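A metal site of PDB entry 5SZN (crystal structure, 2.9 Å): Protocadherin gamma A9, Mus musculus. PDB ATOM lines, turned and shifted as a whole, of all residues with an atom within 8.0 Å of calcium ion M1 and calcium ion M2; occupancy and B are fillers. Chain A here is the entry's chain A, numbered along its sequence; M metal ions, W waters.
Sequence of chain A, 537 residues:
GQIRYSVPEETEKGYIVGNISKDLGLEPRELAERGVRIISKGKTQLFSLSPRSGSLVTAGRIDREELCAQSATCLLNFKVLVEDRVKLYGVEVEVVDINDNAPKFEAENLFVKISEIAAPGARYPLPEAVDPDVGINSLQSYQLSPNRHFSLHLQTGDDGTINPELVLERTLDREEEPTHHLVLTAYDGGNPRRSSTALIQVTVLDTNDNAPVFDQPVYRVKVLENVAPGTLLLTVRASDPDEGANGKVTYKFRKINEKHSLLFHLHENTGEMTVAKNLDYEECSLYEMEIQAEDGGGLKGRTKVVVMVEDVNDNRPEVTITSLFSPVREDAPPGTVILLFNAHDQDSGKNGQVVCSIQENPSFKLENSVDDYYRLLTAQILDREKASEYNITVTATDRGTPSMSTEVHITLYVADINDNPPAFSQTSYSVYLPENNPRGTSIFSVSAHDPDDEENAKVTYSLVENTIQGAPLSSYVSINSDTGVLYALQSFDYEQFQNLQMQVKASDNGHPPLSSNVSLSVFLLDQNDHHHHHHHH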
ATOM      1  N   GLU A 330      -1.889 -24.333   6.899  1.00  0.00           N
ATOM      2  CA  GLU A 330      -0.872 -23.758   6.031  1.00  0.00           C
ATOM      3  C   GLU A 330      -0.545 -24.687   4.858  1.00  0.00           C
ATOM      4  O   GLU A 330      -0.134 -24.216   3.796  1.00  0.00           O
ATOM      5  CB  GLU A 330       0.386 -23.445   6.846  1.00  0.00           C
ATOM      6  CG  GLU A 330       1.480 -22.728   6.081  1.00  0.00           C
ATOM      7  CD  GLU A 330       2.789 -22.725   6.847  1.00  0.00           C
ATOM      8  OE1 GLU A 330       2.851 -23.345   7.924  1.00  0.00           O
ATOM      9  OE2 GLU A 330       3.757 -22.092   6.365  1.00  0.00           O
ATOM     10  N   ASP A 331      -0.733 -25.989   5.039  1.00  0.00           N
ATOM     11  CA  ASP A 331      -0.457 -26.975   4.002  1.00  0.00           C
ATOM     12  C   ASP A 331      -1.546 -27.065   2.944  1.00  0.00           C
ATOM     13  O   ASP A 331      -1.517 -27.984   2.115  1.00  0.00           O
ATOM     14  CB  ASP A 331      -0.252 -28.358   4.639  1.00  0.00           C
ATOM     15  CG  ASP A 331      -1.434 -28.797   5.499  1.00  0.00           C
ATOM     16  OD1 ASP A 331      -2.595 -28.504   5.135  1.00  0.00           O
ATOM     17  OD2 ASP A 331      -1.199 -29.454   6.540  1.00  0.00           O
ATOM     18  N   ILE A 381       0.111 -21.662  -2.208  1.00  0.00           N
ATOM     19  CA  ILE A 381       0.319 -22.236  -0.886  1.00  0.00           C
ATOM     20  C   ILE A 381       0.628 -21.118   0.096  1.00  0.00           C
ATOM     21  O   ILE A 381       1.404 -20.197  -0.206  1.00  0.00           O
ATOM     22  CB  ILE A 381       1.438 -23.296  -0.911  1.00  0.00           C
ATOM     23  CG1 ILE A 381       0.940 -24.585  -1.577  1.00  0.00           C
ATOM     24  CG2 ILE A 381       1.930 -23.610   0.489  1.00  0.00           C
ATOM     25  CD1 ILE A 381       1.272 -24.686  -3.031  1.00  0.00           C
ATOM     26  N   LEU A 382       0.036 -21.195   1.282  1.00  0.00           N
ATOM     27  CA  LEU A 382       0.242 -20.203   2.323  1.00  0.00           C
ATOM     28  C   LEU A 382       1.488 -20.513   3.137  1.00  0.00           C
ATOM     29  O   LEU A 382       2.033 -21.621   3.099  1.00  0.00           O
ATOM     30  CB  LEU A 382      -0.981 -20.119   3.245  1.00  0.00           C
ATOM     31  CG  LEU A 382      -2.281 -19.539   2.674  1.00  0.00           C
ATOM     32  CD1 LEU A 382      -1.995 -18.266   1.896  1.00  0.00           C
ATOM     33  CD2 LEU A 382      -3.025 -20.545   1.801  1.00  0.00           C
ATOM     34  N   ASP A 383       1.953 -19.511   3.883  1.00  0.00           N
ATOM     35  CA  ASP A 383       3.164 -19.648   4.684  1.00  0.00           C
ATOM     36  C   ASP A 383       3.099 -18.602   5.799  1.00  0.00           C
ATOM     37  O   ASP A 383       3.415 -17.433   5.566  1.00  0.00           O
ATOM     38  CB  ASP A 383       4.416 -19.471   3.832  1.00  0.00           C
ATOM     39  CG  ASP A 383       5.690 -19.472   4.643  1.00  0.00           C
ATOM     40  OD1 ASP A 383       5.798 -20.296   5.579  1.00  0.00           O
ATOM     41  OD2 ASP A 383       6.578 -18.653   4.359  1.00  0.00           O
ATOM     42  N   ARG A 384       2.690 -19.022   6.991  1.00  0.00           N
ATOM     43  CA  ARG A 384       2.417 -18.086   8.068  1.00  0.00           C
ATOM     44  C   ARG A 384       3.682 -17.477   8.673  1.00  0.00           C
ATOM     45  O   ARG A 384       3.562 -16.563   9.506  1.00  0.00           O
ATOM     46  CB  ARG A 384       1.607 -18.762   9.174  1.00  0.00           C
ATOM     47  CG  ARG A 384       2.298 -19.932   9.829  1.00  0.00           C
ATOM     48  CD  ARG A 384       1.482 -20.437  10.996  1.00  0.00           C
ATOM     49  NE  ARG A 384       1.341 -19.427  12.043  1.00  0.00           N
ATOM     50  CZ  ARG A 384       2.191 -19.274  13.057  1.00  0.00           C
ATOM     51  NH1 ARG A 384       3.255 -20.064  13.157  1.00  0.00           N
ATOM     52  NH2 ARG A 384       1.982 -18.337  13.969  1.00  0.00           N
ATOM     53  N   GLU A 385       4.865 -17.956   8.304  1.00  0.00           N
ATOM     54  CA  GLU A 385       6.094 -17.310   8.752  1.00  0.00           C
ATOM     55  C   GLU A 385       6.417 -16.062   7.938  1.00  0.00           C
ATOM     56  O   GLU A 385       7.304 -15.300   8.340  1.00  0.00           O
ATOM     57  CB  GLU A 385       7.260 -18.289   8.710  1.00  0.00           C
ATOM     58  CG  GLU A 385       7.309 -19.240   9.892  1.00  0.00           C
ATOM     59  CD  GLU A 385       6.223 -20.300   9.849  1.00  0.00           C
ATOM     60  OE1 GLU A 385       5.898 -20.778   8.751  1.00  0.00           O
ATOM     61  OE2 GLU A 385       5.686 -20.653  10.932  1.00  0.00           O
ATOM     62  N   LYS A 386       5.747 -15.856   6.809  1.00  0.00           N
ATOM     63  CA  LYS A 386       5.833 -14.614   6.055  1.00  0.00           C
ATOM     64  C   LYS A 386       4.586 -13.748   6.168  1.00  0.00           C
ATOM     65  O   LYS A 386       4.694 -12.524   6.072  1.00  0.00           O
ATOM     66  CB  LYS A 386       6.098 -14.901   4.569  1.00  0.00           C
ATOM     67  N   ALA A 415      -3.680 -21.153   9.939  1.00  0.00           N
ATOM     68  CA  ALA A 415      -3.295 -21.993  11.056  1.00  0.00           C
ATOM     69  C   ALA A 415      -1.838 -22.417  10.925  1.00  0.00           C
ATOM     70  O   ALA A 415      -1.167 -22.168   9.916  1.00  0.00           O
ATOM     71  CB  ALA A 415      -4.198 -23.225  11.131  1.00  0.00           C
ATOM     72  N   ASP A 416      -1.336 -23.077  11.968  1.00  0.00           N
ATOM     73  CA  ASP A 416       0.071 -23.444  12.062  1.00  0.00           C
ATOM     74  C   ASP A 416       0.225 -24.945  11.824  1.00  0.00           C
ATOM     75  O   ASP A 416      -0.294 -25.756  12.597  1.00  0.00           O
ATOM     76  CB  ASP A 416       0.664 -23.066  13.419  1.00  0.00           C
ATOM     77  CG  ASP A 416       2.154 -23.327  13.505  1.00  0.00           C
ATOM     78  OD1 ASP A 416       2.817 -23.369  12.449  1.00  0.00           O
ATOM     79  OD2 ASP A 416       2.673 -23.505  14.629  1.00  0.00           O
ATOM     80  N   ILE A 417       0.944 -25.296  10.770  1.00  0.00           N
ATOM     81  CA  ILE A 417       1.362 -26.672  10.495  1.00  0.00           C
ATOM     82  C   ILE A 417       2.860 -26.748  10.712  1.00  0.00           C
ATOM     83  O   ILE A 417       3.613 -25.897  10.213  1.00  0.00           O
ATOM     84  CB  ILE A 417       0.973 -27.105   9.069  1.00  0.00           C
ATOM     85  CG1 ILE A 417      -0.555 -27.125   8.915  1.00  0.00           C
ATOM     86  CG2 ILE A 417       1.551 -28.473   8.753  1.00  0.00           C
ATOM     87  CD1 ILE A 417      -1.248 -28.047   9.893  1.00  0.00           C
ATOM     88  N   ASN A 418       3.303 -27.760  11.458  1.00  0.00           N
ATOM     89  CA  ASN A 418       4.689 -27.867  11.901  1.00  0.00           C
ATOM     90  C   ASN A 418       5.559 -28.354  10.741  1.00  0.00           C
ATOM     91  O   ASN A 418       5.611 -29.547  10.443  1.00  0.00           O
ATOM     92  CB  ASN A 418       4.789 -28.809  13.094  1.00  0.00           C
ATOM     93  CG  ASN A 418       6.170 -28.806  13.713  1.00  0.00           C
ATOM     94  OD1 ASN A 418       7.004 -27.947  13.419  1.00  0.00           O
ATOM     95  ND2 ASN A 418       6.428 -29.773  14.597  1.00  0.00           N
ATOM     96  N   ASP A 419       6.254 -27.422  10.095  1.00  0.00           N
ATOM     97  CA  ASP A 419       7.213 -27.746   9.045  1.00  0.00           C
ATOM     98  C   ASP A 419       8.549 -27.055   9.248  1.00  0.00           C
ATOM     99  O   ASP A 419       9.386 -27.075   8.339  1.00  0.00           O
ATOM    100  CB  ASP A 419       6.635 -27.387   7.669  1.00  0.00           C
ATOM    101  CG  ASP A 419       6.235 -25.925   7.562  1.00  0.00           C
ATOM    102  OD1 ASP A 419       5.847 -25.348   8.589  1.00  0.00           O
ATOM    103  OD2 ASP A 419       6.314 -25.368   6.450  1.00  0.00           O
ATOM    104  N   ASN A 420       8.790 -26.455  10.415  1.00  0.00           N
ATOM    105  CA  ASN A 420      10.039 -25.755  10.706  1.00  0.00           C
ATOM    106  C   ASN A 420      10.678 -26.347  11.944  1.00  0.00           C
ATOM    107  O   ASN A 420      10.061 -26.331  13.025  1.00  0.00           O
ATOM    108  CB  ASN A 420       9.786 -24.261  10.887  1.00  0.00           C
ATOM    109  CG  ASN A 420       9.272 -23.602   9.622  1.00  0.00           C
ATOM    110  OD1 ASN A 420       9.566 -24.044   8.518  1.00  0.00           O
ATOM    111  ND2 ASN A 420       8.501 -22.530   9.791  1.00  0.00           N
ATOM    112  N   ASP A 450      12.355 -21.745  17.497  1.00  0.00           N
ATOM    113  CA  ASP A 450      11.545 -22.434  16.497  1.00  0.00           C
ATOM    114  C   ASP A 450      10.608 -21.426  15.837  1.00  0.00           C
ATOM    115  O   ASP A 450       9.910 -20.681  16.538  1.00  0.00           O
ATOM    116  CB  ASP A 450      10.756 -23.578  17.131  1.00  0.00           C
ATOM    117  CG  ASP A 450      10.175 -24.537  16.099  1.00  0.00           C
ATOM    118  OD1 ASP A 450       9.577 -24.073  15.110  1.00  0.00           O
ATOM    119  OD2 ASP A 450      10.305 -25.768  16.296  1.00  0.00           O
ATOM    120  N   PRO A 451      10.568 -21.357  14.501  1.00  0.00           N
ATOM    121  CA  PRO A 451       9.718 -20.364  13.850  1.00  0.00           C
ATOM    122  C   PRO A 451       8.229 -20.575  14.052  1.00  0.00           C
ATOM    123  O   PRO A 451       7.468 -19.605  13.999  1.00  0.00           O
ATOM    124  CB  PRO A 451      10.097 -20.497  12.365  1.00  0.00           C
ATOM    125  CG  PRO A 451      11.443 -21.130  12.369  1.00  0.00           C
ATOM    126  CD  PRO A 451      11.453 -22.057  13.545  1.00  0.00           C
ATOM    127  N   ASP A 452       7.794 -21.812  14.288  1.00  0.00           N
ATOM    128  CA  ASP A 452       6.363 -22.100  14.422  1.00  0.00           C
ATOM    129  C   ASP A 452       5.824 -21.478  15.713  1.00  0.00           C
ATOM    130  O   ASP A 452       6.508 -20.738  16.420  1.00  0.00           O
ATOM    131  CB  ASP A 452       6.127 -23.613  14.379  1.00  0.00           C
ATOM    132  CG  ASP A 452       6.371 -24.202  13.011  1.00  0.00           C
ATOM    133  OD1 ASP A 452       6.254 -23.456  12.013  1.00  0.00           O
ATOM    134  OD2 ASP A 452       6.675 -25.402  12.926  1.00  0.00           O
ATOM    135  N   ASP A 453       4.568 -21.781  16.026  1.00  0.00           N
ATOM    136  CA  ASP A 453       3.899 -21.170  17.163  1.00  0.00           C
ATOM    137  C   ASP A 453       3.379 -22.250  18.113  1.00  0.00           C
ATOM    138  O   ASP A 453       3.069 -23.369  17.690  1.00  0.00           O
ATOM    139  CB  ASP A 453       2.739 -20.275  16.717  1.00  0.00           C
ATOM    140  CG  ASP A 453       2.196 -19.419  17.844  1.00  0.00           C
ATOM    141  OD1 ASP A 453       2.852 -19.341  18.910  1.00  0.00           O
ATOM    142  OD2 ASP A 453       1.123 -18.806  17.668  1.00  0.00           O
ATOM    143  N   ASN A 456       4.454 -26.368  18.628  1.00  0.00           N
ATOM    144  CA  ASN A 456       5.445 -26.602  17.578  1.00  0.00           C
ATOM    145  C   ASN A 456       6.619 -25.642  17.658  1.00  0.00           C
ATOM    146  O   ASN A 456       7.452 -25.598  16.742  1.00  0.00           O
ATOM    147  CB  ASN A 456       4.776 -26.512  16.210  1.00  0.00           C
ATOM    148  CG  ASN A 456       3.633 -27.504  16.063  1.00  0.00           C
ATOM    149  OD1 ASN A 456       3.584 -28.523  16.743  1.00  0.00           O
ATOM    150  ND2 ASN A 456       2.702 -27.195  15.157  1.00  0.00           N
HETATM  151 CA    CA M   1       4.369 -23.037  10.560  1.00  0.00          CA
HETATM  152 CA    CA M   2       5.329 -23.231   7.525  1.00  0.00          CA
HETATM  153 CA    CA M   3       8.494 -26.711  14.908  1.00  0.00          CA
HETATM  154  O   HOH W   1       7.231 -21.536   6.758  1.00  0.00           O
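OE2 of Glu 330 lies close to N of Arg 384.
The side-chain carboxylate (OD2) of Asp 452 lies within hydrogen-bond range of the backbone NH (N) of Asn 420 (3.4 Å).
OD2 of Asp 452 sits close to OD1 of Asn 418 (2.6 Å).
The backbone NH (N) of Asp 452 lies close to the side-chain carboxylate (OD1) of Asp 450 (3.0 Å).
The side-chain carboxylate (OD2) of Asp 416 is in salt-bridge range of the guanidinium group (NH1) of Arg 384, at 3.8 Å.
The backbone NH (N) of Asp 453 sits at hydrogen-bond distance from the side-chain carboxylate (OD2) of Asp 416 (2.9 Å).
The guanidinium group (NH1) of Arg 384 lies close to the side-chain carboxylate (OE2) of Glu 385, at 3.3 Å.
The guanidinium group (NH2) of Arg 384 lies within salt-bridge range of the side-chain carboxylate (OD2) of Asp 453 (3.8 Å).
Arg 384 touches calcium ion M1 (CG to CA, 3.8 Å).
Within 4 Å of calcium ion M1: Glu 330, Arg 384, Glu 385, Asp 416, Ile 417, Asp 419 and Asp 452.
Along chain A the residues within 4 Å of calcium ion M1 span positions 330 to 452.
The nearest printed residue that does not touch calcium ion M1 is Asn 420 (4.2 Å).
Merely in contact with calcium ion M2: Asp 383 (3.6 Å) and Asn 420 (3.96 Å).
Within 4 Å of calcium ion M2: Glu 330, Asp 383, Glu 385, Asp 419 and Asn 420.
Calcium ion M1 is bound by OD1 of Asp 452 (2.4 Å).
Calcium ion M1 is bound by OD1 of Asp 416 (2.5 Å).
OE2 of Glu 385 is bound to calcium ion M1 (2.7 Å).
Slightly farther from calcium ion M1 lies O of Ile 417 (3.0 Å).
Slightly farther from calcium ion M1 lies the side-chain carboxylate (OE1) of Glu 330 (3.1 Å).
Calcium ion M2 is bound by the side-chain carboxylate (OE2) of Glu 330, the side-chain carboxylate (OD1) of Asp 419, the side-chain carboxylate (OE1) of Glu 330, the side-chain carboxylate (OD2) of Asp 419, water W1 and the side-chain carboxylate (OE1) of Glu 385.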
